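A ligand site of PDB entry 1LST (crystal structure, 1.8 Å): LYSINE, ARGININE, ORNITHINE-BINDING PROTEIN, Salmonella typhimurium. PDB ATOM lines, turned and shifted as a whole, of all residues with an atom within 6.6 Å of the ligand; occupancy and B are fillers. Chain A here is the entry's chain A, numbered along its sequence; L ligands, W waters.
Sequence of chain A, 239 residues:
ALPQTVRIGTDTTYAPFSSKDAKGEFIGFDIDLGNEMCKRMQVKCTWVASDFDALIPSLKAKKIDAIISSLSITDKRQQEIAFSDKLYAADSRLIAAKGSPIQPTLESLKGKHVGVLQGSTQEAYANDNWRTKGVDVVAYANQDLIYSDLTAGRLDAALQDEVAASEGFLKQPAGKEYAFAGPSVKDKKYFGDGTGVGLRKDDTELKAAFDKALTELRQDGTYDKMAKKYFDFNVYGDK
OH of Tyr 14 lies within hydrogen-bond range of N of Asp 161 (3.0 Å). OG of Ser 120 lies close to OE1 of Gln 122, at 3.4 Å. NE2 of Gln 122 sits at hydrogen-bond distance from OG of Ser 92 (2.8 Å). OG1 of Thr 74 sits at hydrogen-bond distance from N of Arg 77 (3.1 Å). OD1 of Asp 161 is in hydrogen-bond range of NE2 of Gln 122, 2.9 Å away. N of Asp 11 lies within hydrogen-bond range of OG of Ser 69 (2.9 Å). O of Leu 117 sits at hydrogen-bond distance from OG of Ser 120, at 2.6 Å. The guanidinium group (NH2) of Arg 77 lies within hydrogen-bond range of the backbone carbonyl oxygen (O) of Gly 119, at 3.4 Å.
O1 of the ligand sits at hydrogen-bond distance from N of Thr 121, 2.9 Å away. OD2 of Asp 11 lies within salt-bridge range of N2 of the ligand (2.8 Å). OD2 of Asp 161 is in salt-bridge range of N1 of the ligand, at 3.0 Å. The side-chain hydroxyl (OG) of Ser 72 is in hydrogen-bond range of a nitrogen (N1) of the ligand, 3.1 Å away. O2 of the ligand is in salt-bridge range of NH1 of Arg 77, 2.8 Å away. The backbone carbonyl oxygen (O) of Ser 70 lies within hydrogen-bond range of a nitrogen (N1) of the ligand. N of Ser 72 sits at hydrogen-bond distance from O2 of the ligand, 2.9 Å away.
Tyr 14 touches the ligand (CG to N2, 3.5 Å). CE1 of Phe 52 touches C6 of the ligand (3.6 Å). Ser 69 touches the ligand (O to C6, 3.3 Å). Leu 71 touches the ligand. Leu 117 touches the ligand. Ser 120 touches the ligand (CA to O1, 3.2 Å). Gln 122 touches the ligand (OE1 to C3, 3.5 Å). Hydrophobic or aromatic side chains within 4 Å of the ligand: Tyr 14, Phe 52 and Leu 117. Within 4 Å of the ligand: Asp 11, Tyr 14, Phe 52, Ser 69, Ser 70, Leu 71, Ser 72, Arg 77, Leu 117, Ser 120, Thr 121, Gln 122 and Asp 161. Along chain A the residues within 4 Å of the ligand span positions 11 to 161. The nearest printed residue that does not touch the ligand is Gly 119 (4.5 Å).
Water W1 lies within hydrogen-bond range of N2 of the ligand (2.7 Å), O of Asp 11 (2.8 Å) and OG of Ser 69 (2.9 Å).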
ATOM      1  N   ASP A  11       1.459  -3.688   1.920  1.00  0.00           N
ATOM      2  CA  ASP A  11       0.613  -4.872   1.936  1.00  0.00           C
ATOM      3  C   ASP A  11      -0.021  -4.843   3.313  1.00  0.00           C
ATOM      4  O   ASP A  11       0.584  -5.104   4.373  1.00  0.00           O
ATOM      5  CB  ASP A  11       1.505  -6.089   1.735  1.00  0.00           C
ATOM      6  CG  ASP A  11       0.921  -7.411   2.211  1.00  0.00           C
ATOM      7  OD1 ASP A  11      -0.295  -7.579   2.232  1.00  0.00           O
ATOM      8  OD2 ASP A  11       1.700  -8.266   2.586  1.00  0.00           O
ATOM      9  N   THR A  12      -1.331  -4.599   3.278  1.00  0.00           N
ATOM     10  CA  THR A  12      -2.094  -4.412   4.501  1.00  0.00           C
ATOM     11  C   THR A  12      -2.546  -5.680   5.213  1.00  0.00           C
ATOM     12  O   THR A  12      -3.645  -5.695   5.771  1.00  0.00           O
ATOM     13  CB  THR A  12      -3.299  -3.487   4.140  1.00  0.00           C
ATOM     14  OG1 THR A  12      -4.002  -3.996   3.019  1.00  0.00           O
ATOM     15  CG2 THR A  12      -2.791  -2.083   3.834  1.00  0.00           C
ATOM     16  N   THR A  13      -1.768  -6.762   5.196  1.00  0.00           N
ATOM     17  CA  THR A  13      -2.127  -7.982   5.911  1.00  0.00           C
ATOM     18  C   THR A  13      -0.971  -8.389   6.840  1.00  0.00           C
ATOM     19  O   THR A  13      -0.651  -9.569   6.968  1.00  0.00           O
ATOM     20  CB  THR A  13      -2.471  -9.130   4.880  1.00  0.00           C
ATOM     21  OG1 THR A  13      -1.339  -9.360   4.074  1.00  0.00           O
ATOM     22  CG2 THR A  13      -3.634  -8.790   4.010  1.00  0.00           C
ATOM     23  N   TYR A  14      -0.322  -7.441   7.503  1.00  0.00           N
ATOM     24  CA  TYR A  14       0.790  -7.774   8.369  1.00  0.00           C
ATOM     25  C   TYR A  14       0.740  -6.928   9.648  1.00  0.00           C
ATOM     26  O   TYR A  14       1.575  -6.050   9.921  1.00  0.00           O
ATOM     27  CB  TYR A  14       2.042  -7.537   7.571  1.00  0.00           C
ATOM     28  CG  TYR A  14       3.120  -8.591   7.694  1.00  0.00           C
ATOM     29  CD1 TYR A  14       2.928  -9.892   7.261  1.00  0.00           C
ATOM     30  CD2 TYR A  14       4.335  -8.211   8.237  1.00  0.00           C
ATOM     31  CE1 TYR A  14       3.966 -10.814   7.337  1.00  0.00           C
ATOM     32  CE2 TYR A  14       5.365  -9.129   8.323  1.00  0.00           C
ATOM     33  CZ  TYR A  14       5.180 -10.420   7.855  1.00  0.00           C
ATOM     34  OH  TYR A  14       6.255 -11.304   7.905  1.00  0.00           O
ATOM     35  N   PHE A  52       1.996  -8.302  -1.377  1.00  0.00           N
ATOM     36  CA  PHE A  52       3.418  -8.175  -1.151  1.00  0.00           C
ATOM     37  C   PHE A  52       4.303  -8.467  -2.369  1.00  0.00           C
ATOM     38  O   PHE A  52       5.224  -7.708  -2.645  1.00  0.00           O
ATOM     39  CB  PHE A  52       3.832  -9.088  -0.019  1.00  0.00           C
ATOM     40  CG  PHE A  52       5.273  -8.805   0.436  1.00  0.00           C
ATOM     41  CD1 PHE A  52       5.554  -7.631   1.147  1.00  0.00           C
ATOM     42  CD2 PHE A  52       6.299  -9.667   0.122  1.00  0.00           C
ATOM     43  CE1 PHE A  52       6.833  -7.355   1.548  1.00  0.00           C
ATOM     44  CE2 PHE A  52       7.591  -9.381   0.529  1.00  0.00           C
ATOM     45  CZ  PHE A  52       7.857  -8.234   1.249  1.00  0.00           C
ATOM     46  N   LEU A  55       4.823  -5.583  -4.964  1.00  0.00           N
ATOM     47  CA  LEU A  55       5.359  -4.290  -4.567  1.00  0.00           C
ATOM     48  C   LEU A  55       6.633  -3.855  -5.283  1.00  0.00           C
ATOM     49  O   LEU A  55       6.704  -2.757  -5.865  1.00  0.00           O
ATOM     50  CB  LEU A  55       5.577  -4.301  -3.054  1.00  0.00           C
ATOM     51  CG  LEU A  55       4.309  -4.276  -2.163  1.00  0.00           C
ATOM     52  CD1 LEU A  55       4.763  -4.518  -0.758  1.00  0.00           C
ATOM     53  CD2 LEU A  55       3.557  -2.949  -2.192  1.00  0.00           C
ATOM     54  N   SER A  69       6.621  -1.641   3.978  1.00  0.00           N
ATOM     55  CA  SER A  69       5.821  -2.843   4.147  1.00  0.00           C
ATOM     56  C   SER A  69       6.662  -3.917   4.829  1.00  0.00           C
ATOM     57  O   SER A  69       6.705  -5.065   4.379  1.00  0.00           O
ATOM     58  CB  SER A  69       5.351  -3.247   2.720  1.00  0.00           C
ATOM     59  OG  SER A  69       4.214  -4.115   2.664  1.00  0.00           O
ATOM     60  N   SER A  70       7.365  -3.586   5.921  1.00  0.00           N
ATOM     61  CA  SER A  70       8.279  -4.507   6.593  1.00  0.00           C
ATOM     62  C   SER A  70       9.259  -5.154   5.595  1.00  0.00           C
ATOM     63  O   SER A  70       9.618  -6.336   5.706  1.00  0.00           O
ATOM     64  CB  SER A  70       7.500  -5.604   7.369  1.00  0.00           C
ATOM     65  OG  SER A  70       6.577  -5.054   8.319  1.00  0.00           O
ATOM     66  N   LEU A  71       9.741  -4.331   4.635  1.00  0.00           N
ATOM     67  CA  LEU A  71      10.600  -4.828   3.567  1.00  0.00           C
ATOM     68  C   LEU A  71      12.034  -4.967   4.015  1.00  0.00           C
ATOM     69  O   LEU A  71      12.721  -3.963   4.197  1.00  0.00           O
ATOM     70  CB  LEU A  71      10.523  -3.884   2.349  1.00  0.00           C
ATOM     71  CG  LEU A  71      11.160  -4.377   1.046  1.00  0.00           C
ATOM     72  CD1 LEU A  71      10.301  -5.536   0.472  1.00  0.00           C
ATOM     73  CD2 LEU A  71      11.276  -3.209   0.031  1.00  0.00           C
ATOM     74  N   SER A  72      12.502  -6.195   4.255  1.00  0.00           N
ATOM     75  CA  SER A  72      13.861  -6.438   4.700  1.00  0.00           C
ATOM     76  C   SER A  72      14.907  -6.022   3.663  1.00  0.00           C
ATOM     77  O   SER A  72      14.719  -6.250   2.477  1.00  0.00           O
ATOM     78  CB  SER A  72      14.039  -7.911   5.011  1.00  0.00           C
ATOM     79  OG  SER A  72      13.274  -8.236   6.175  1.00  0.00           O
ATOM     80  N   ILE A  73      15.987  -5.429   4.164  1.00  0.00           N
ATOM     81  CA  ILE A  73      17.118  -4.953   3.390  1.00  0.00           C
ATOM     82  C   ILE A  73      18.026  -6.149   3.202  1.00  0.00           C
ATOM     83  O   ILE A  73      18.701  -6.601   4.151  1.00  0.00           O
ATOM     84  CB  ILE A  73      17.882  -3.816   4.163  1.00  0.00           C
ATOM     85  CG1 ILE A  73      16.905  -2.719   4.556  1.00  0.00           C
ATOM     86  CG2 ILE A  73      19.034  -3.271   3.274  1.00  0.00           C
ATOM     87  CD1 ILE A  73      17.563  -1.700   5.513  1.00  0.00           C
ATOM     88  N   THR A  74      18.041  -6.723   2.006  1.00  0.00           N
ATOM     89  CA  THR A  74      18.871  -7.911   1.756  1.00  0.00           C
ATOM     90  C   THR A  74      19.811  -7.600   0.616  1.00  0.00           C
ATOM     91  O   THR A  74      19.507  -6.757  -0.245  1.00  0.00           O
ATOM     92  CB  THR A  74      18.017  -9.148   1.357  1.00  0.00           C
ATOM     93  OG1 THR A  74      17.409  -8.838   0.097  1.00  0.00           O
ATOM     94  CG2 THR A  74      16.963  -9.494   2.378  1.00  0.00           C
ATOM     95  N   ARG A  77      17.861  -7.979  -2.843  1.00  0.00           N
ATOM     96  CA  ARG A  77      17.061  -6.811  -3.168  1.00  0.00           C
ATOM     97  C   ARG A  77      17.874  -5.553  -3.500  1.00  0.00           C
ATOM     98  O   ARG A  77      17.447  -4.767  -4.347  1.00  0.00           O
ATOM     99  CB  ARG A  77      16.106  -6.531  -1.998  1.00  0.00           C
ATOM    100  CG  ARG A  77      14.959  -7.515  -2.023  1.00  0.00           C
ATOM    101  CD  ARG A  77      14.184  -7.415  -0.744  1.00  0.00           C
ATOM    102  NE  ARG A  77      13.081  -8.348  -0.748  1.00  0.00           N
ATOM    103  CZ  ARG A  77      12.383  -8.655   0.338  1.00  0.00           C
ATOM    104  NH1 ARG A  77      12.686  -8.078   1.521  1.00  0.00           N
ATOM    105  NH2 ARG A  77      11.364  -9.523   0.241  1.00  0.00           N
ATOM    106  N   ALA A  90      13.990  -7.089  12.089  1.00  0.00           N
ATOM    107  CA  ALA A  90      12.977  -8.066  11.799  1.00  0.00           C
ATOM    108  C   ALA A  90      13.634  -9.440  11.719  1.00  0.00           C
ATOM    109  O   ALA A  90      14.440  -9.686  10.796  1.00  0.00           O
ATOM    110  CB  ALA A  90      12.312  -7.744  10.472  1.00  0.00           C
ATOM    111  N   SER A  92      13.040 -13.818  11.746  1.00  0.00           N
ATOM    112  CA  SER A  92      12.043 -14.793  11.327  1.00  0.00           C
ATOM    113  C   SER A  92      11.867 -15.875  12.383  1.00  0.00           C
ATOM    114  O   SER A  92      12.862 -16.287  13.007  1.00  0.00           O
ATOM    115  CB  SER A  92      12.457 -15.460  10.013  1.00  0.00           C
ATOM    116  OG  SER A  92      12.190 -14.573   8.956  1.00  0.00           O
ATOM    117  N   LEU A 117       4.691 -16.530   2.990  1.00  0.00           N
ATOM    118  CA  LEU A 117       4.154 -15.477   2.126  1.00  0.00           C
ATOM    119  C   LEU A 117       4.918 -15.452   0.796  1.00  0.00           C
ATOM    120  O   LEU A 117       6.137 -15.376   0.787  1.00  0.00           O
ATOM    121  CB  LEU A 117       4.269 -14.122   2.851  1.00  0.00           C
ATOM    122  CG  LEU A 117       3.892 -12.825   2.128  1.00  0.00           C
ATOM    123  CD1 LEU A 117       2.409 -12.822   1.765  1.00  0.00           C
ATOM    124  CD2 LEU A 117       4.193 -11.641   3.074  1.00  0.00           C
ATOM    125  N   GLY A 119       6.752 -14.083  -2.154  1.00  0.00           N
ATOM    126  CA  GLY A 119       7.571 -12.919  -2.443  1.00  0.00           C
ATOM    127  C   GLY A 119       8.443 -12.570  -1.258  1.00  0.00           C
ATOM    128  O   GLY A 119       9.301 -11.690  -1.409  1.00  0.00           O
ATOM    129  N   SER A 120       8.317 -13.238  -0.085  1.00  0.00           N
ATOM    130  CA  SER A 120       9.084 -12.902   1.099  1.00  0.00           C
ATOM    131  C   SER A 120      10.445 -13.558   1.167  1.00  0.00           C
ATOM    132  O   SER A 120      10.741 -14.544   0.477  1.00  0.00           O
ATOM    133  CB  SER A 120       8.266 -13.281   2.339  1.00  0.00           C
ATOM    134  OG  SER A 120       8.098 -14.696   2.412  1.00  0.00           O
ATOM    135  N   THR A 121      11.275 -13.060   2.070  1.00  0.00           N
ATOM    136  CA  THR A 121      12.567 -13.675   2.349  1.00  0.00           C
ATOM    137  C   THR A 121      12.312 -15.071   2.955  1.00  0.00           C
ATOM    138  O   THR A 121      13.084 -16.005   2.713  1.00  0.00           O
ATOM    139  CB  THR A 121      13.345 -12.829   3.330  1.00  0.00           C
ATOM    140  OG1 THR A 121      12.491 -12.676   4.452  1.00  0.00           O
ATOM    141  CG2 THR A 121      13.746 -11.461   2.790  1.00  0.00           C
ATOM    142  N   GLN A 122      11.215 -15.275   3.707  1.00  0.00           N
ATOM    143  CA  GLN A 122      10.840 -16.581   4.258  1.00  0.00           C
ATOM    144  C   GLN A 122      10.547 -17.590   3.152  1.00  0.00           C
ATOM    145  O   GLN A 122      10.969 -18.735   3.285  1.00  0.00           O
ATOM    146  CB  GLN A 122       9.609 -16.470   5.142  1.00  0.00           C
ATOM    147  CG  GLN A 122       9.840 -15.733   6.474  1.00  0.00           C
ATOM    148  CD  GLN A 122       9.660 -14.213   6.403  1.00  0.00           C
ATOM    149  OE1 GLN A 122       9.083 -13.647   5.470  1.00  0.00           O
ATOM    150  NE2 GLN A 122      10.148 -13.539   7.414  1.00  0.00           N
ATOM    151  N   GLN A 143      -0.577 -12.845   4.311  1.00  0.00           N
ATOM    152  CA  GLN A 143      -0.379 -13.505   5.605  1.00  0.00           C
ATOM    153  C   GLN A 143      -1.647 -13.895   6.371  1.00  0.00           C
ATOM    154  O   GLN A 143      -1.671 -14.876   7.135  1.00  0.00           O
ATOM    155  CB  GLN A 143       0.471 -12.598   6.474  1.00  0.00           C
ATOM    156  CG  GLN A 143       0.964 -13.152   7.805  1.00  0.00           C
ATOM    157  CD  GLN A 143       1.942 -14.313   7.711  1.00  0.00           C
ATOM    158  OE1 GLN A 143       1.936 -15.216   8.578  1.00  0.00           O
ATOM    159  NE2 GLN A 143       2.834 -14.324   6.745  1.00  0.00           N
ATOM    160  N   GLN A 160       7.345 -16.483   9.256  1.00  0.00           N
ATOM    161  CA  GLN A 160       7.068 -15.082   8.928  1.00  0.00           C
ATOM    162  C   GLN A 160       7.913 -14.267   9.916  1.00  0.00           C
ATOM    163  O   GLN A 160       8.660 -14.880  10.716  1.00  0.00           O
ATOM    164  CB  GLN A 160       5.592 -14.693   9.147  1.00  0.00           C
ATOM    165  CG  GLN A 160       5.005 -14.911  10.578  1.00  0.00           C
ATOM    166  CD  GLN A 160       4.825 -16.409  10.872  1.00  0.00           C
ATOM    167  OE1 GLN A 160       4.032 -17.059  10.200  1.00  0.00           O
ATOM    168  NE2 GLN A 160       5.541 -17.044  11.799  1.00  0.00           N
ATOM    169  N   ASP A 161       7.864 -12.913   9.865  1.00  0.00           N
ATOM    170  CA  ASP A 161       8.592 -12.111  10.844  1.00  0.00           C
ATOM    171  C   ASP A 161       8.007 -12.350  12.239  1.00  0.00           C
ATOM    172  O   ASP A 161       6.796 -12.371  12.483  1.00  0.00           O
ATOM    173  CB  ASP A 161       8.486 -10.619  10.496  1.00  0.00           C
ATOM    174  CG  ASP A 161       9.204 -10.159   9.221  1.00  0.00           C
ATOM    175  OD1 ASP A 161      10.029 -10.893   8.638  1.00  0.00           O
ATOM    176  OD2 ASP A 161       8.931  -9.034   8.816  1.00  0.00           O
ATOM    177  N   PHE A 191      17.761 -13.318   5.351  1.00  0.00           N
ATOM    178  CA  PHE A 191      16.815 -12.467   6.009  1.00  0.00           C
ATOM    179  C   PHE A 191      17.247 -11.034   6.054  1.00  0.00           C
ATOM    180  O   PHE A 191      16.421 -10.182   6.420  1.00  0.00           O
ATOM    181  CB  PHE A 191      16.558 -13.056   7.415  1.00  0.00           C
ATOM    182  CG  PHE A 191      15.910 -14.449   7.303  1.00  0.00           C
ATOM    183  CD1 PHE A 191      14.702 -14.633   6.637  1.00  0.00           C
ATOM    184  CD2 PHE A 191      16.537 -15.549   7.871  1.00  0.00           C
ATOM    185  CE1 PHE A 191      14.153 -15.912   6.542  1.00  0.00           C
ATOM    186  CE2 PHE A 191      15.980 -16.817   7.775  1.00  0.00           C
ATOM    187  CZ  PHE A 191      14.784 -16.991   7.114  1.00  0.00           C
ATOM    188  N   THR A 195      14.450  -3.656   8.267  1.00  0.00           N
ATOM    189  CA  THR A 195      13.547  -3.277   7.176  1.00  0.00           C
ATOM    190  C   THR A 195      13.809  -1.821   6.784  1.00  0.00           C
ATOM    191  O   THR A 195      14.335  -1.066   7.622  1.00  0.00           O
ATOM    192  CB  THR A 195      12.053  -3.420   7.594  1.00  0.00           C
ATOM    193  OG1 THR A 195      11.707  -2.453   8.591  1.00  0.00           O
ATOM    194  CG2 THR A 195      11.806  -4.861   8.084  1.00  0.00           C
HETATM  195  N1  LIG L   1      10.243  -9.075   6.145  1.00  0.00           N
HETATM  196  C1  LIG L   1       9.845 -10.093   5.205  1.00  0.00           C
HETATM  197  C2  LIG L   1      10.369  -9.698   3.802  1.00  0.00           C
HETATM  198  O1  LIG L   1      10.198 -10.456   2.841  1.00  0.00           O
HETATM  199  C3  LIG L   1       8.329 -10.204   5.200  1.00  0.00           C
HETATM  200  C4  LIG L   1       7.575  -8.897   5.020  1.00  0.00           C
HETATM  201  C5  LIG L   1       6.149  -9.239   4.703  1.00  0.00           C
HETATM  202  C6  LIG L   1       5.306  -7.985   4.730  1.00  0.00           C
HETATM  203  N2  LIG L   1       3.925  -8.248   4.312  1.00  0.00           N
HETATM  204  O2  LIG L   1      10.945  -8.612   3.680  1.00  0.00           O
HETATM  205  O   HOH W   1       3.220  -5.725   4.883  1.00  0.00           O
